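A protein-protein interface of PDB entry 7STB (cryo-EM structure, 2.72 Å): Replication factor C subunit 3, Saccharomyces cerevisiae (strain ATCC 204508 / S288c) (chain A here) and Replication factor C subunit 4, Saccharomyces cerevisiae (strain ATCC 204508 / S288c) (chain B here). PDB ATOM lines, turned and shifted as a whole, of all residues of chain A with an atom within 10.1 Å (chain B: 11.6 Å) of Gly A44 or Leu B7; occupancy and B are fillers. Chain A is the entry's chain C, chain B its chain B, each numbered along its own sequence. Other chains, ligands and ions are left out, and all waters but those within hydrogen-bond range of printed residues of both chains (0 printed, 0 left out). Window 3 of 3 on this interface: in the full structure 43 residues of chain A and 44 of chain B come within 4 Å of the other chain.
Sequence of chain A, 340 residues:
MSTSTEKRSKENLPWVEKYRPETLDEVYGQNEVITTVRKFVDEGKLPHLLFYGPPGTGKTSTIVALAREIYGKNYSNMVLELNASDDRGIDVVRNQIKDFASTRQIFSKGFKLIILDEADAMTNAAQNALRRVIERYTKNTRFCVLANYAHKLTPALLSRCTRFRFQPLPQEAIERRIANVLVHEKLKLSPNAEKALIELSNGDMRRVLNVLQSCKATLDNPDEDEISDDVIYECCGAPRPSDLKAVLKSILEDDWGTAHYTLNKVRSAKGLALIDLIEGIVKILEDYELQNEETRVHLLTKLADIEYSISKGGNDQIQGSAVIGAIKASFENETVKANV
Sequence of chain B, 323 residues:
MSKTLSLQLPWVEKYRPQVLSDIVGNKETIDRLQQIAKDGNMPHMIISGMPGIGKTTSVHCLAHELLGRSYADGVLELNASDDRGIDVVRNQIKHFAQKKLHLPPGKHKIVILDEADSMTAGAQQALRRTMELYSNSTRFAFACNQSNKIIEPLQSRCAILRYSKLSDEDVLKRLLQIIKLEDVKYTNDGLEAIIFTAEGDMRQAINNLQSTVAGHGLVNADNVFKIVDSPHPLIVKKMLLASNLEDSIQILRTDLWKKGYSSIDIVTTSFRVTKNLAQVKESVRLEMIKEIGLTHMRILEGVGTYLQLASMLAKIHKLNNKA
OD1 of Asn A140 sits close to NZ of Lys A139 (3.4 Å). The backbone NH of Lys A45 lies within hydrogen-bond range of the backbone carbonyl oxygen of Phe A40, 2.8 Å away.
Lys A39 touches Ala B214. Gly B215 touches Lys A39. Ser B211 touches Phe A40 (OG to CZ, 3.3 Å). Phe A40 touches Ala B214. OE1 of Glu A43 touches O of Ala B214, 3.8 Å away. Gly A44 touches Leu B7 (O to CA, 3.5 Å). CB of Pro A47 touches NE2 of Gln B210, 3.9 Å away. Thr A138 touches Leu B9. Leu B9 touches Lys A139 (CD2 to CA, 3.6 Å).
Printed residues of chain B within 4 Å of Gly A44: Leu B7. Leu B7 touches one residue of chain A. No residue of chain B comes within 4 Å of Val A41. No residue of chain B comes within 4 Å of Asp A42. Glu A43 touches just one residue of chain B: Ala B214. No residue of chain B comes within 4 Å of Gly A110. Of chain B, only Leu B9 (3.6 Å) comes within 4 Å of Lys A139. Of the printed residues of chain A, Gly B215 touches Lys A39 (3.0 Å). Of the printed residues of chain A, Ala B214 touches Lys A39, Phe A40 and Glu A43. Of the printed residues of chain B, Thr A138 touches Leu B9. Printed residues of chain B within 4 Å of Lys A39: Ala B214 and Gly B215. Of the printed residues of chain A, Ser B211 touches Phe A40 (3.3 Å). The nearest printed residue of chain B that does not touch Gly A44 is Gln B8 (4.001 Å). The nearest printed residue of chain B that does not touch Lys A39 is Val B213 (7.0 Å).
Of the 24 printed residues of chain A, 7 touch a printed residue of chain B. Hydrophobic or aromatic side chains of chain A within 4 Å of the printed part of chain B: Phe A40 and Pro A47. Of the 13 printed residues of chain B, 6 touch a printed residue of chain A. Hydrophobic or aromatic side chains of chain B that line the printed part of chain A: Leu B9 and Ala B214. Among the printed residues, 9 pairs touch across the chains.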
ATOM      1  N   THR A  36       2.584  -4.131  33.223  1.00  0.00           N
ATOM      2  CA  THR A  36       1.201  -4.579  33.123  1.00  0.00           C
ATOM      3  C   THR A  36       0.493  -3.899  31.958  1.00  0.00           C
ATOM      4  O   THR A  36      -0.249  -4.545  31.208  1.00  0.00           O
ATOM      5  CB  THR A  36       0.467  -4.304  34.437  1.00  0.00           C
ATOM      6  OG1 THR A  36       1.161  -4.943  35.516  1.00  0.00           O
ATOM      7  CG2 THR A  36      -0.954  -4.834  34.378  1.00  0.00           C
ATOM      8  N   VAL A  37       0.718  -2.595  31.781  1.00  0.00           N
ATOM      9  CA  VAL A  37       0.071  -1.877  30.685  1.00  0.00           C
ATOM     10  C   VAL A  37       0.625  -2.334  29.339  1.00  0.00           C
ATOM     11  O   VAL A  37      -0.120  -2.447  28.355  1.00  0.00           O
ATOM     12  CB  VAL A  37       0.226  -0.358  30.883  1.00  0.00           C
ATOM     13  CG1 VAL A  37      -0.349   0.390  29.698  1.00  0.00           C
ATOM     14  CG2 VAL A  37      -0.468   0.081  32.163  1.00  0.00           C
ATOM     15  N   ARG A  38       1.934  -2.595  29.266  1.00  0.00           N
ATOM     16  CA  ARG A  38       2.508  -3.143  28.040  1.00  0.00           C
ATOM     17  C   ARG A  38       1.829  -4.453  27.669  1.00  0.00           C
ATOM     18  O   ARG A  38       1.460  -4.668  26.510  1.00  0.00           O
ATOM     19  CB  ARG A  38       4.013  -3.377  28.196  1.00  0.00           C
ATOM     20  CG  ARG A  38       4.873  -2.160  28.489  1.00  0.00           C
ATOM     21  CD  ARG A  38       4.965  -1.191  27.328  1.00  0.00           C
ATOM     22  NE  ARG A  38       5.798  -0.050  27.691  1.00  0.00           N
ATOM     23  CZ  ARG A  38       7.112   0.009  27.508  1.00  0.00           C
ATOM     24  NH1 ARG A  38       7.775  -0.971  26.918  1.00  0.00           N
ATOM     25  NH2 ARG A  38       7.779   1.076  27.937  1.00  0.00           N
ATOM     26  N   LYS A  39       1.674  -5.351  28.644  1.00  0.00           N
ATOM     27  CA  LYS A  39       1.028  -6.629  28.363  1.00  0.00           C
ATOM     28  C   LYS A  39      -0.421  -6.427  27.940  1.00  0.00           C
ATOM     29  O   LYS A  39      -0.900  -7.079  27.004  1.00  0.00           O
ATOM     30  CB  LYS A  39       1.114  -7.539  29.587  1.00  0.00           C
ATOM     31  CG  LYS A  39       2.505  -8.102  29.832  1.00  0.00           C
ATOM     32  CD  LYS A  39       2.546  -8.975  31.075  1.00  0.00           C
ATOM     33  CE  LYS A  39       3.954  -9.477  31.358  1.00  0.00           C
ATOM     34  NZ  LYS A  39       4.527 -10.228  30.206  1.00  0.00           N
ATOM     35  N   PHE A  40      -1.131  -5.519  28.613  1.00  0.00           N
ATOM     36  CA  PHE A  40      -2.518  -5.248  28.250  1.00  0.00           C
ATOM     37  C   PHE A  40      -2.624  -4.801  26.797  1.00  0.00           C
ATOM     38  O   PHE A  40      -3.458  -5.309  26.039  1.00  0.00           O
ATOM     39  CB  PHE A  40      -3.107  -4.180  29.177  1.00  0.00           C
ATOM     40  CG  PHE A  40      -3.627  -4.712  30.490  1.00  0.00           C
ATOM     41  CD1 PHE A  40      -4.242  -5.952  30.574  1.00  0.00           C
ATOM     42  CD2 PHE A  40      -3.509  -3.955  31.644  1.00  0.00           C
ATOM     43  CE1 PHE A  40      -4.720  -6.424  31.781  1.00  0.00           C
ATOM     44  CE2 PHE A  40      -3.986  -4.424  32.852  1.00  0.00           C
ATOM     45  CZ  PHE A  40      -4.590  -5.659  32.921  1.00  0.00           C
ATOM     46  N   VAL A  41      -1.787  -3.844  26.389  1.00  0.00           N
ATOM     47  CA  VAL A  41      -1.882  -3.329  25.026  1.00  0.00           C
ATOM     48  C   VAL A  41      -1.436  -4.383  24.021  1.00  0.00           C
ATOM     49  O   VAL A  41      -2.029  -4.521  22.943  1.00  0.00           O
ATOM     50  CB  VAL A  41      -1.077  -2.023  24.875  1.00  0.00           C
ATOM     51  CG1 VAL A  41      -1.653  -0.941  25.773  1.00  0.00           C
ATOM     52  CG2 VAL A  41       0.398  -2.247  25.172  1.00  0.00           C
ATOM     53  N   ASP A  42      -0.389  -5.145  24.346  1.00  0.00           N
ATOM     54  CA  ASP A  42       0.096  -6.163  23.420  1.00  0.00           C
ATOM     55  C   ASP A  42      -0.959  -7.235  23.182  1.00  0.00           C
ATOM     56  O   ASP A  42      -1.154  -7.682  22.046  1.00  0.00           O
ATOM     57  CB  ASP A  42       1.384  -6.787  23.956  1.00  0.00           C
ATOM     58  CG  ASP A  42       1.980  -7.803  23.003  1.00  0.00           C
ATOM     59  OD1 ASP A  42       2.035  -7.518  21.788  1.00  0.00           O
ATOM     60  OD2 ASP A  42       2.392  -8.887  23.467  1.00  0.00           O
ATOM     61  N   GLU A  43      -1.647  -7.661  24.238  1.00  0.00           N
ATOM     62  CA  GLU A  43      -2.706  -8.653  24.116  1.00  0.00           C
ATOM     63  C   GLU A  43      -4.058  -8.035  23.786  1.00  0.00           C
ATOM     64  O   GLU A  43      -5.036  -8.773  23.625  1.00  0.00           O
ATOM     65  CB  GLU A  43      -2.817  -9.467  25.409  1.00  0.00           C
ATOM     66  CG  GLU A  43      -1.560 -10.254  25.751  1.00  0.00           C
ATOM     67  CD  GLU A  43      -1.682 -11.004  27.062  1.00  0.00           C
ATOM     68  OE1 GLU A  43      -2.771 -10.968  27.672  1.00  0.00           O
ATOM     69  OE2 GLU A  43      -0.687 -11.631  27.483  1.00  0.00           O
ATOM     70  N   GLY A  44      -4.139  -6.712  23.680  1.00  0.00           N
ATOM     71  CA  GLY A  44      -5.406  -6.068  23.374  1.00  0.00           C
ATOM     72  C   GLY A  44      -6.474  -6.324  24.415  1.00  0.00           C
ATOM     73  O   GLY A  44      -7.632  -6.581  24.064  1.00  0.00           O
ATOM     74  N   LYS A  45      -6.109  -6.260  25.692  1.00  0.00           N
ATOM     75  CA  LYS A  45      -7.021  -6.516  26.803  1.00  0.00           C
ATOM     76  C   LYS A  45      -6.863  -5.442  27.872  1.00  0.00           C
ATOM     77  O   LYS A  45      -6.783  -5.724  29.070  1.00  0.00           O
ATOM     78  CB  LYS A  45      -6.776  -7.905  27.387  1.00  0.00           C
ATOM     79  CG  LYS A  45      -7.253  -9.040  26.495  1.00  0.00           C
ATOM     80  CD  LYS A  45      -6.760 -10.394  26.988  1.00  0.00           C
ATOM     81  CE  LYS A  45      -7.340 -10.750  28.348  1.00  0.00           C
ATOM     82  NZ  LYS A  45      -6.855 -12.073  28.828  1.00  0.00           N
ATOM     83  N   LEU A  46      -6.815  -4.187  27.444  1.00  0.00           N
ATOM     84  CA  LEU A  46      -6.671  -3.076  28.376  1.00  0.00           C
ATOM     85  C   LEU A  46      -8.008  -2.795  29.052  1.00  0.00           C
ATOM     86  O   LEU A  46      -8.988  -2.506  28.359  1.00  0.00           O
ATOM     87  CB  LEU A  46      -6.182  -1.831  27.647  1.00  0.00           C
ATOM     88  CG  LEU A  46      -5.781  -0.651  28.531  1.00  0.00           C
ATOM     89  CD1 LEU A  46      -4.501  -0.962  29.292  1.00  0.00           C
ATOM     90  CD2 LEU A  46      -5.621   0.611  27.700  1.00  0.00           C
ATOM     91  N   PRO A  47      -8.099  -2.868  30.378  1.00  0.00           N
ATOM     92  CA  PRO A  47      -9.353  -2.554  31.062  1.00  0.00           C
ATOM     93  C   PRO A  47      -9.414  -1.089  31.480  1.00  0.00           C
ATOM     94  O   PRO A  47      -8.447  -0.336  31.354  1.00  0.00           O
ATOM     95  CB  PRO A  47      -9.306  -3.472  32.287  1.00  0.00           C
ATOM     96  CG  PRO A  47      -7.848  -3.542  32.623  1.00  0.00           C
ATOM     97  CD  PRO A  47      -7.076  -3.344  31.329  1.00  0.00           C
ATOM     98  N   ILE A  70      -0.166   3.624  21.608  1.00  0.00           N
ATOM     99  CA  ILE A  70      -1.287   2.902  21.010  1.00  0.00           C
ATOM    100  C   ILE A  70      -1.602   3.453  19.624  1.00  0.00           C
ATOM    101  O   ILE A  70      -1.795   2.694  18.667  1.00  0.00           O
ATOM    102  CB  ILE A  70      -2.518   2.961  21.933  1.00  0.00           C
ATOM    103  CG1 ILE A  70      -2.221   2.255  23.259  1.00  0.00           C
ATOM    104  CG2 ILE A  70      -3.727   2.329  21.251  1.00  0.00           C
ATOM    105  CD1 ILE A  70      -3.270   2.483  24.328  1.00  0.00           C
ATOM    106  N   GLN A 105     -14.964   4.624  14.930  1.00  0.00           N
ATOM    107  CA  GLN A 105     -13.538   4.903  14.957  1.00  0.00           C
ATOM    108  C   GLN A 105     -13.083   5.493  13.626  1.00  0.00           C
ATOM    109  O   GLN A 105     -13.635   5.184  12.567  1.00  0.00           O
ATOM    110  CB  GLN A 105     -12.750   3.627  15.252  1.00  0.00           C
ATOM    111  CG  GLN A 105     -11.378   3.882  15.830  1.00  0.00           C
ATOM    112  CD  GLN A 105     -11.454   4.346  17.267  1.00  0.00           C
ATOM    113  OE1 GLN A 105     -11.403   5.541  17.549  1.00  0.00           O
ATOM    114  NE2 GLN A 105     -11.587   3.399  18.185  1.00  0.00           N
ATOM    115  N   SER A 108     -10.221   2.488  13.049  1.00  0.00           N
ATOM    116  CA  SER A 108     -10.305   1.229  13.788  1.00  0.00           C
ATOM    117  C   SER A 108      -9.042   0.994  14.613  1.00  0.00           C
ATOM    118  O   SER A 108      -8.519  -0.121  14.678  1.00  0.00           O
ATOM    119  CB  SER A 108     -10.561   0.055  12.841  1.00  0.00           C
ATOM    120  OG  SER A 108     -10.820  -1.136  13.564  1.00  0.00           O
ATOM    121  N   LYS A 109      -8.548   2.054  15.251  1.00  0.00           N
ATOM    122  CA  LYS A 109      -7.333   1.967  16.052  1.00  0.00           C
ATOM    123  C   LYS A 109      -7.628   1.405  17.437  1.00  0.00           C
ATOM    124  O   LYS A 109      -7.284   2.020  18.451  1.00  0.00           O
ATOM    125  CB  LYS A 109      -6.676   3.344  16.173  1.00  0.00           C
ATOM    126  CG  LYS A 109      -6.276   3.963  14.841  1.00  0.00           C
ATOM    127  CD  LYS A 109      -4.955   3.402  14.339  1.00  0.00           C
ATOM    128  CE  LYS A 109      -3.773   3.995  15.090  1.00  0.00           C
ATOM    129  NZ  LYS A 109      -2.486   3.775  14.374  1.00  0.00           N
ATOM    130  N   GLY A 110      -8.265   0.238  17.489  1.00  0.00           N
ATOM    131  CA  GLY A 110      -8.526  -0.428  18.749  1.00  0.00           C
ATOM    132  C   GLY A 110      -9.715   0.132  19.502  1.00  0.00           C
ATOM    133  O   GLY A 110     -10.772  -0.502  19.561  1.00  0.00           O
ATOM    134  N   PHE A 111      -9.557   1.318  20.081  1.00  0.00           N
ATOM    135  CA  PHE A 111     -10.608   1.914  20.893  1.00  0.00           C
ATOM    136  C   PHE A 111     -10.309   3.395  21.076  1.00  0.00           C
ATOM    137  O   PHE A 111      -9.231   3.881  20.729  1.00  0.00           O
ATOM    138  CB  PHE A 111     -10.727   1.208  22.247  1.00  0.00           C
ATOM    139  CG  PHE A 111      -9.424   1.095  22.986  1.00  0.00           C
ATOM    140  CD1 PHE A 111      -8.994   2.114  23.818  1.00  0.00           C
ATOM    141  CD2 PHE A 111      -8.629  -0.029  22.846  1.00  0.00           C
ATOM    142  CE1 PHE A 111      -7.795   2.013  24.497  1.00  0.00           C
ATOM    143  CE2 PHE A 111      -7.430  -0.135  23.523  1.00  0.00           C
ATOM    144  CZ  PHE A 111      -7.012   0.887  24.350  1.00  0.00           C
ATOM    145  N   LYS A 112     -11.288   4.105  21.630  1.00  0.00           N
ATOM    146  CA  LYS A 112     -11.172   5.524  21.935  1.00  0.00           C
ATOM    147  C   LYS A 112     -10.923   5.688  23.427  1.00  0.00           C
ATOM    148  O   LYS A 112     -11.632   5.098  24.247  1.00  0.00           O
ATOM    149  CB  LYS A 112     -12.436   6.280  21.523  1.00  0.00           C
ATOM    150  CG  LYS A 112     -12.802   6.118  20.058  1.00  0.00           C
ATOM    151  CD  LYS A 112     -14.191   6.659  19.757  1.00  0.00           C
ATOM    152  CE  LYS A 112     -14.188   8.171  19.634  1.00  0.00           C
ATOM    153  NZ  LYS A 112     -15.467   8.681  19.071  1.00  0.00           N
ATOM    154  N   THR A 138     -18.244   0.261  26.163  1.00  0.00           N
ATOM    155  CA  THR A 138     -16.968  -0.360  26.488  1.00  0.00           C
ATOM    156  C   THR A 138     -16.408  -1.218  25.364  1.00  0.00           C
ATOM    157  O   THR A 138     -15.230  -1.583  25.427  1.00  0.00           O
ATOM    158  CB  THR A 138     -17.094  -1.224  27.755  1.00  0.00           C
ATOM    159  OG1 THR A 138     -15.832  -1.832  28.052  1.00  0.00           O
ATOM    160  CG2 THR A 138     -18.148  -2.307  27.570  1.00  0.00           C
ATOM    161  N   LYS A 139     -17.205  -1.551  24.347  1.00  0.00           N
ATOM    162  CA  LYS A 139     -16.690  -2.344  23.235  1.00  0.00           C
ATOM    163  C   LYS A 139     -15.602  -1.593  22.479  1.00  0.00           C
ATOM    164  O   LYS A 139     -14.575  -2.176  22.114  1.00  0.00           O
ATOM    165  CB  LYS A 139     -17.833  -2.722  22.292  1.00  0.00           C
ATOM    166  CG  LYS A 139     -17.427  -3.670  21.176  1.00  0.00           C
ATOM    167  CD  LYS A 139     -18.582  -3.935  20.224  1.00  0.00           C
ATOM    168  CE  LYS A 139     -18.168  -4.858  19.088  1.00  0.00           C
ATOM    169  NZ  LYS A 139     -17.065  -4.286  18.268  1.00  0.00           N
ATOM    170  N   ASN A 140     -15.806  -0.298  22.235  1.00  0.00           N
ATOM    171  CA  ASN A 140     -14.858   0.516  21.480  1.00  0.00           C
ATOM    172  C   ASN A 140     -14.628   1.849  22.176  1.00  0.00           C
ATOM    173  O   ASN A 140     -14.567   2.903  21.536  1.00  0.00           O
ATOM    174  CB  ASN A 140     -15.342   0.739  20.048  1.00  0.00           C
ATOM    175  CG  ASN A 140     -15.604  -0.559  19.314  1.00  0.00           C
ATOM    176  OD1 ASN A 140     -16.738  -1.037  19.260  1.00  0.00           O
ATOM    177  ND2 ASN A 140     -14.555  -1.139  18.744  1.00  0.00           N
ATOM    178  N   THR A 141     -14.497   1.820  23.499  1.00  0.00           N
ATOM    179  CA  THR A 141     -14.202   3.023  24.264  1.00  0.00           C
ATOM    180  C   THR A 141     -13.569   2.608  25.583  1.00  0.00           C
ATOM    181  O   THR A 141     -13.953   1.592  26.166  1.00  0.00           O
ATOM    182  CB  THR A 141     -15.463   3.857  24.516  1.00  0.00           C
ATOM    183  OG1 THR A 141     -15.969   4.352  23.272  1.00  0.00           O
ATOM    184  CG2 THR A 141     -15.153   5.031  25.433  1.00  0.00           C
ATOM    185  N   ARG A 142     -12.602   3.398  26.042  1.00  0.00           N
ATOM    186  CA  ARG A 142     -11.875   3.092  27.262  1.00  0.00           C
ATOM    187  C   ARG A 142     -11.789   4.345  28.118  1.00  0.00           C
ATOM    188  O   ARG A 142     -11.777   5.466  27.602  1.00  0.00           O
ATOM    189  CB  ARG A 142     -10.472   2.555  26.950  1.00  0.00           C
ATOM    190  CG  ARG A 142      -9.670   2.126  28.165  1.00  0.00           C
ATOM    191  CD  ARG A 142     -10.374   1.001  28.901  1.00  0.00           C
ATOM    192  NE  ARG A 142     -10.570  -0.163  28.045  1.00  0.00           N
ATOM    193  CZ  ARG A 142     -11.419  -1.149  28.299  1.00  0.00           C
ATOM    194  NH1 ARG A 142     -12.167  -1.154  29.391  1.00  0.00           N
ATOM    195  NH2 ARG A 142     -11.520  -2.157  27.438  1.00  0.00           N
ATOM    196  N   LEU B   7      -9.721  -6.771  20.086  1.00  0.00           N
ATOM    197  CA  LEU B   7      -9.986  -6.303  21.442  1.00  0.00           C
ATOM    198  C   LEU B   7     -11.235  -6.972  22.009  1.00  0.00           C
ATOM    199  O   LEU B   7     -12.345  -6.459  21.868  1.00  0.00           O
ATOM    200  CB  LEU B   7     -10.148  -4.782  21.462  1.00  0.00           C
ATOM    201  N   GLN B   8     -11.043  -8.121  22.650  1.00  0.00           N
ATOM    202  CA  GLN B   8     -12.160  -8.851  23.232  1.00  0.00           C
ATOM    203  C   GLN B   8     -12.768  -8.070  24.390  1.00  0.00           C
ATOM    204  O   GLN B   8     -12.077  -7.353  25.120  1.00  0.00           O
ATOM    205  CB  GLN B   8     -11.702 -10.228  23.712  1.00  0.00           C
ATOM    206  CG  GLN B   8     -12.841 -11.172  24.060  1.00  0.00           C
ATOM    207  CD  GLN B   8     -12.349 -12.526  24.531  1.00  0.00           C
ATOM    208  OE1 GLN B   8     -12.590 -12.925  25.671  1.00  0.00           O
ATOM    209  NE2 GLN B   8     -11.656 -13.242  23.653  1.00  0.00           N
ATOM    210  N   LEU B   9     -14.079  -8.214  24.554  1.00  0.00           N
ATOM    211  CA  LEU B   9     -14.771  -7.507  25.619  1.00  0.00           C
ATOM    212  C   LEU B   9     -14.308  -8.024  26.980  1.00  0.00           C
ATOM    213  O   LEU B   9     -14.012  -9.214  27.125  1.00  0.00           O
ATOM    214  CB  LEU B   9     -16.284  -7.684  25.487  1.00  0.00           C
ATOM    215  CG  LEU B   9     -17.014  -6.660  24.616  1.00  0.00           C
ATOM    216  CD1 LEU B   9     -18.432  -7.124  24.327  1.00  0.00           C
ATOM    217  CD2 LEU B   9     -17.025  -5.292  25.282  1.00  0.00           C
ATOM    218  N   PRO B  10     -14.227  -7.161  27.994  1.00  0.00           N
ATOM    219  CA  PRO B  10     -13.885  -7.645  29.337  1.00  0.00           C
ATOM    220  C   PRO B  10     -14.912  -8.649  29.839  1.00  0.00           C
ATOM    221  O   PRO B  10     -16.097  -8.583  29.503  1.00  0.00           O
ATOM    222  CB  PRO B  10     -13.877  -6.375  30.195  1.00  0.00           C
ATOM    223  CG  PRO B  10     -13.798  -5.236  29.257  1.00  0.00           C
ATOM    224  CD  PRO B  10     -14.244  -5.690  27.906  1.00  0.00           C
ATOM    225  N   TRP B  11     -14.440  -9.594  30.656  1.00  0.00           N
ATOM    226  CA  TRP B  11     -15.311 -10.662  31.134  1.00  0.00           C
ATOM    227  C   TRP B  11     -16.435 -10.147  32.022  1.00  0.00           C
ATOM    228  O   TRP B  11     -17.433 -10.853  32.206  1.00  0.00           O
ATOM    229  CB  TRP B  11     -14.494 -11.714  31.885  1.00  0.00           C
ATOM    230  CG  TRP B  11     -13.387 -12.302  31.067  1.00  0.00           C
ATOM    231  CD1 TRP B  11     -13.360 -12.448  29.711  1.00  0.00           C
ATOM    232  CD2 TRP B  11     -12.150 -12.839  31.552  1.00  0.00           C
ATOM    233  NE1 TRP B  11     -12.182 -13.035  29.321  1.00  0.00           N
ATOM    234  CE2 TRP B  11     -11.423 -13.287  30.433  1.00  0.00           C
ATOM    235  CE3 TRP B  11     -11.588 -12.984  32.824  1.00  0.00           C
ATOM    236  CZ2 TRP B  11     -10.162 -13.867  30.545  1.00  0.00           C
ATOM    237  CZ3 TRP B  11     -10.336 -13.561  32.933  1.00  0.00           C
ATOM    238  CH2 TRP B  11      -9.637 -13.994  31.801  1.00  0.00           C
ATOM    239  N   GLU B  13     -18.436  -7.954  31.166  1.00  0.00           N
ATOM    240  CA  GLU B  13     -19.529  -7.822  30.213  1.00  0.00           C
ATOM    241  C   GLU B  13     -19.695  -9.042  29.319  1.00  0.00           C
ATOM    242  O   GLU B  13     -20.824  -9.357  28.927  1.00  0.00           O
ATOM    243  CB  GLU B  13     -19.313  -6.586  29.332  1.00  0.00           C
ATOM    244  CG  GLU B  13     -19.387  -5.269  30.089  1.00  0.00           C
ATOM    245  CD  GLU B  13     -20.775  -4.979  30.626  1.00  0.00           C
ATOM    246  OE1 GLU B  13     -21.763  -5.394  29.983  1.00  0.00           O
ATOM    247  OE2 GLU B  13     -20.879  -4.339  31.693  1.00  0.00           O
ATOM    248  N   LYS B  14     -18.603  -9.734  28.983  1.00  0.00           N
ATOM    249  CA  LYS B  14     -18.710 -10.909  28.125  1.00  0.00           C
ATOM    250  C   LYS B  14     -19.532 -12.006  28.791  1.00  0.00           C
ATOM    251  O   LYS B  14     -20.376 -12.640  28.145  1.00  0.00           O
ATOM    252  CB  LYS B  14     -17.317 -11.426  27.769  1.00  0.00           C
ATOM    253  CG  LYS B  14     -17.317 -12.619  26.825  1.00  0.00           C
ATOM    254  CD  LYS B  14     -15.909 -13.139  26.586  1.00  0.00           C
ATOM    255  CE  LYS B  14     -15.920 -14.410  25.752  1.00  0.00           C
ATOM    256  NZ  LYS B  14     -14.555 -14.975  25.572  1.00  0.00           N
ATOM    257  N   GLU B 182     -13.168 -20.054  30.475  1.00  0.00           N
ATOM    258  CA  GLU B 182     -12.010 -19.430  29.848  1.00  0.00           C
ATOM    259  C   GLU B 182     -10.766 -20.308  29.876  1.00  0.00           C
ATOM    260  O   GLU B 182      -9.750 -19.929  29.284  1.00  0.00           O
ATOM    261  CB  GLU B 182     -11.695 -18.097  30.536  1.00  0.00           C
ATOM    262  CG  GLU B 182     -12.633 -16.962  30.154  1.00  0.00           C
ATOM    263  CD  GLU B 182     -12.374 -16.433  28.756  1.00  0.00           C
ATOM    264  OE1 GLU B 182     -11.267 -16.660  28.225  1.00  0.00           O
ATOM    265  OE2 GLU B 182     -13.281 -15.789  28.187  1.00  0.00           O
ATOM    266  N   GLN B 210      -9.222 -10.952  35.892  1.00  0.00           N
ATOM    267  CA  GLN B 210      -8.812 -10.726  34.511  1.00  0.00           C
ATOM    268  C   GLN B 210      -7.475  -9.997  34.455  1.00  0.00           C
ATOM    269  O   GLN B 210      -6.581 -10.368  33.684  1.00  0.00           O
ATOM    270  CB  GLN B 210      -9.885  -9.929  33.769  1.00  0.00           C
ATOM    271  CG  GLN B 210      -9.617  -9.766  32.279  1.00  0.00           C
ATOM    272  CD  GLN B 210     -10.063  -8.419  31.751  1.00  0.00           C
ATOM    273  OE1 GLN B 210     -10.945  -8.336  30.896  1.00  0.00           O
ATOM    274  NE2 GLN B 210      -9.459  -7.355  32.261  1.00  0.00           N
ATOM    275  N   SER B 211      -7.320  -8.953  35.270  1.00  0.00           N
ATOM    276  CA  SER B 211      -6.062  -8.217  35.278  1.00  0.00           C
ATOM    277  C   SER B 211      -4.907  -9.119  35.686  1.00  0.00           C
ATOM    278  O   SER B 211      -3.837  -9.089  35.065  1.00  0.00           O
ATOM    279  CB  SER B 211      -6.164  -7.015  36.215  1.00  0.00           C
ATOM    280  OG  SER B 211      -4.979  -6.239  36.178  1.00  0.00           O
ATOM    281  N   VAL B 213      -4.624 -12.456  35.477  1.00  0.00           N
ATOM    282  CA  VAL B 213      -4.293 -13.468  34.478  1.00  0.00           C
ATOM    283  C   VAL B 213      -3.604 -12.825  33.282  1.00  0.00           C
ATOM    284  O   VAL B 213      -2.654 -13.384  32.722  1.00  0.00           O
ATOM    285  CB  VAL B 213      -5.544 -14.259  34.044  1.00  0.00           C
ATOM    286  CG1 VAL B 213      -6.649 -13.332  33.566  1.00  0.00           C
ATOM    287  CG2 VAL B 213      -5.188 -15.272  32.958  1.00  0.00           C
ATOM    288  N   ALA B 214      -4.063 -11.638  32.870  1.00  0.00           N
ATOM    289  CA  ALA B 214      -3.469 -10.991  31.707  1.00  0.00           C
ATOM    290  C   ALA B 214      -2.078 -10.446  32.007  1.00  0.00           C
ATOM    291  O   ALA B 214      -1.249 -10.340  31.096  1.00  0.00           O
ATOM    292  CB  ALA B 214      -4.380  -9.868  31.213  1.00  0.00           C
ATOM    293  N   GLY B 215      -1.799 -10.100  33.261  1.00  0.00           N
ATOM    294  CA  GLY B 215      -0.514  -9.528  33.605  1.00  0.00           C
ATOM    295  C   GLY B 215       0.548 -10.553  33.947  1.00  0.00           C
ATOM    296  O   GLY B 215       1.714 -10.383  33.579  1.00  0.00           O
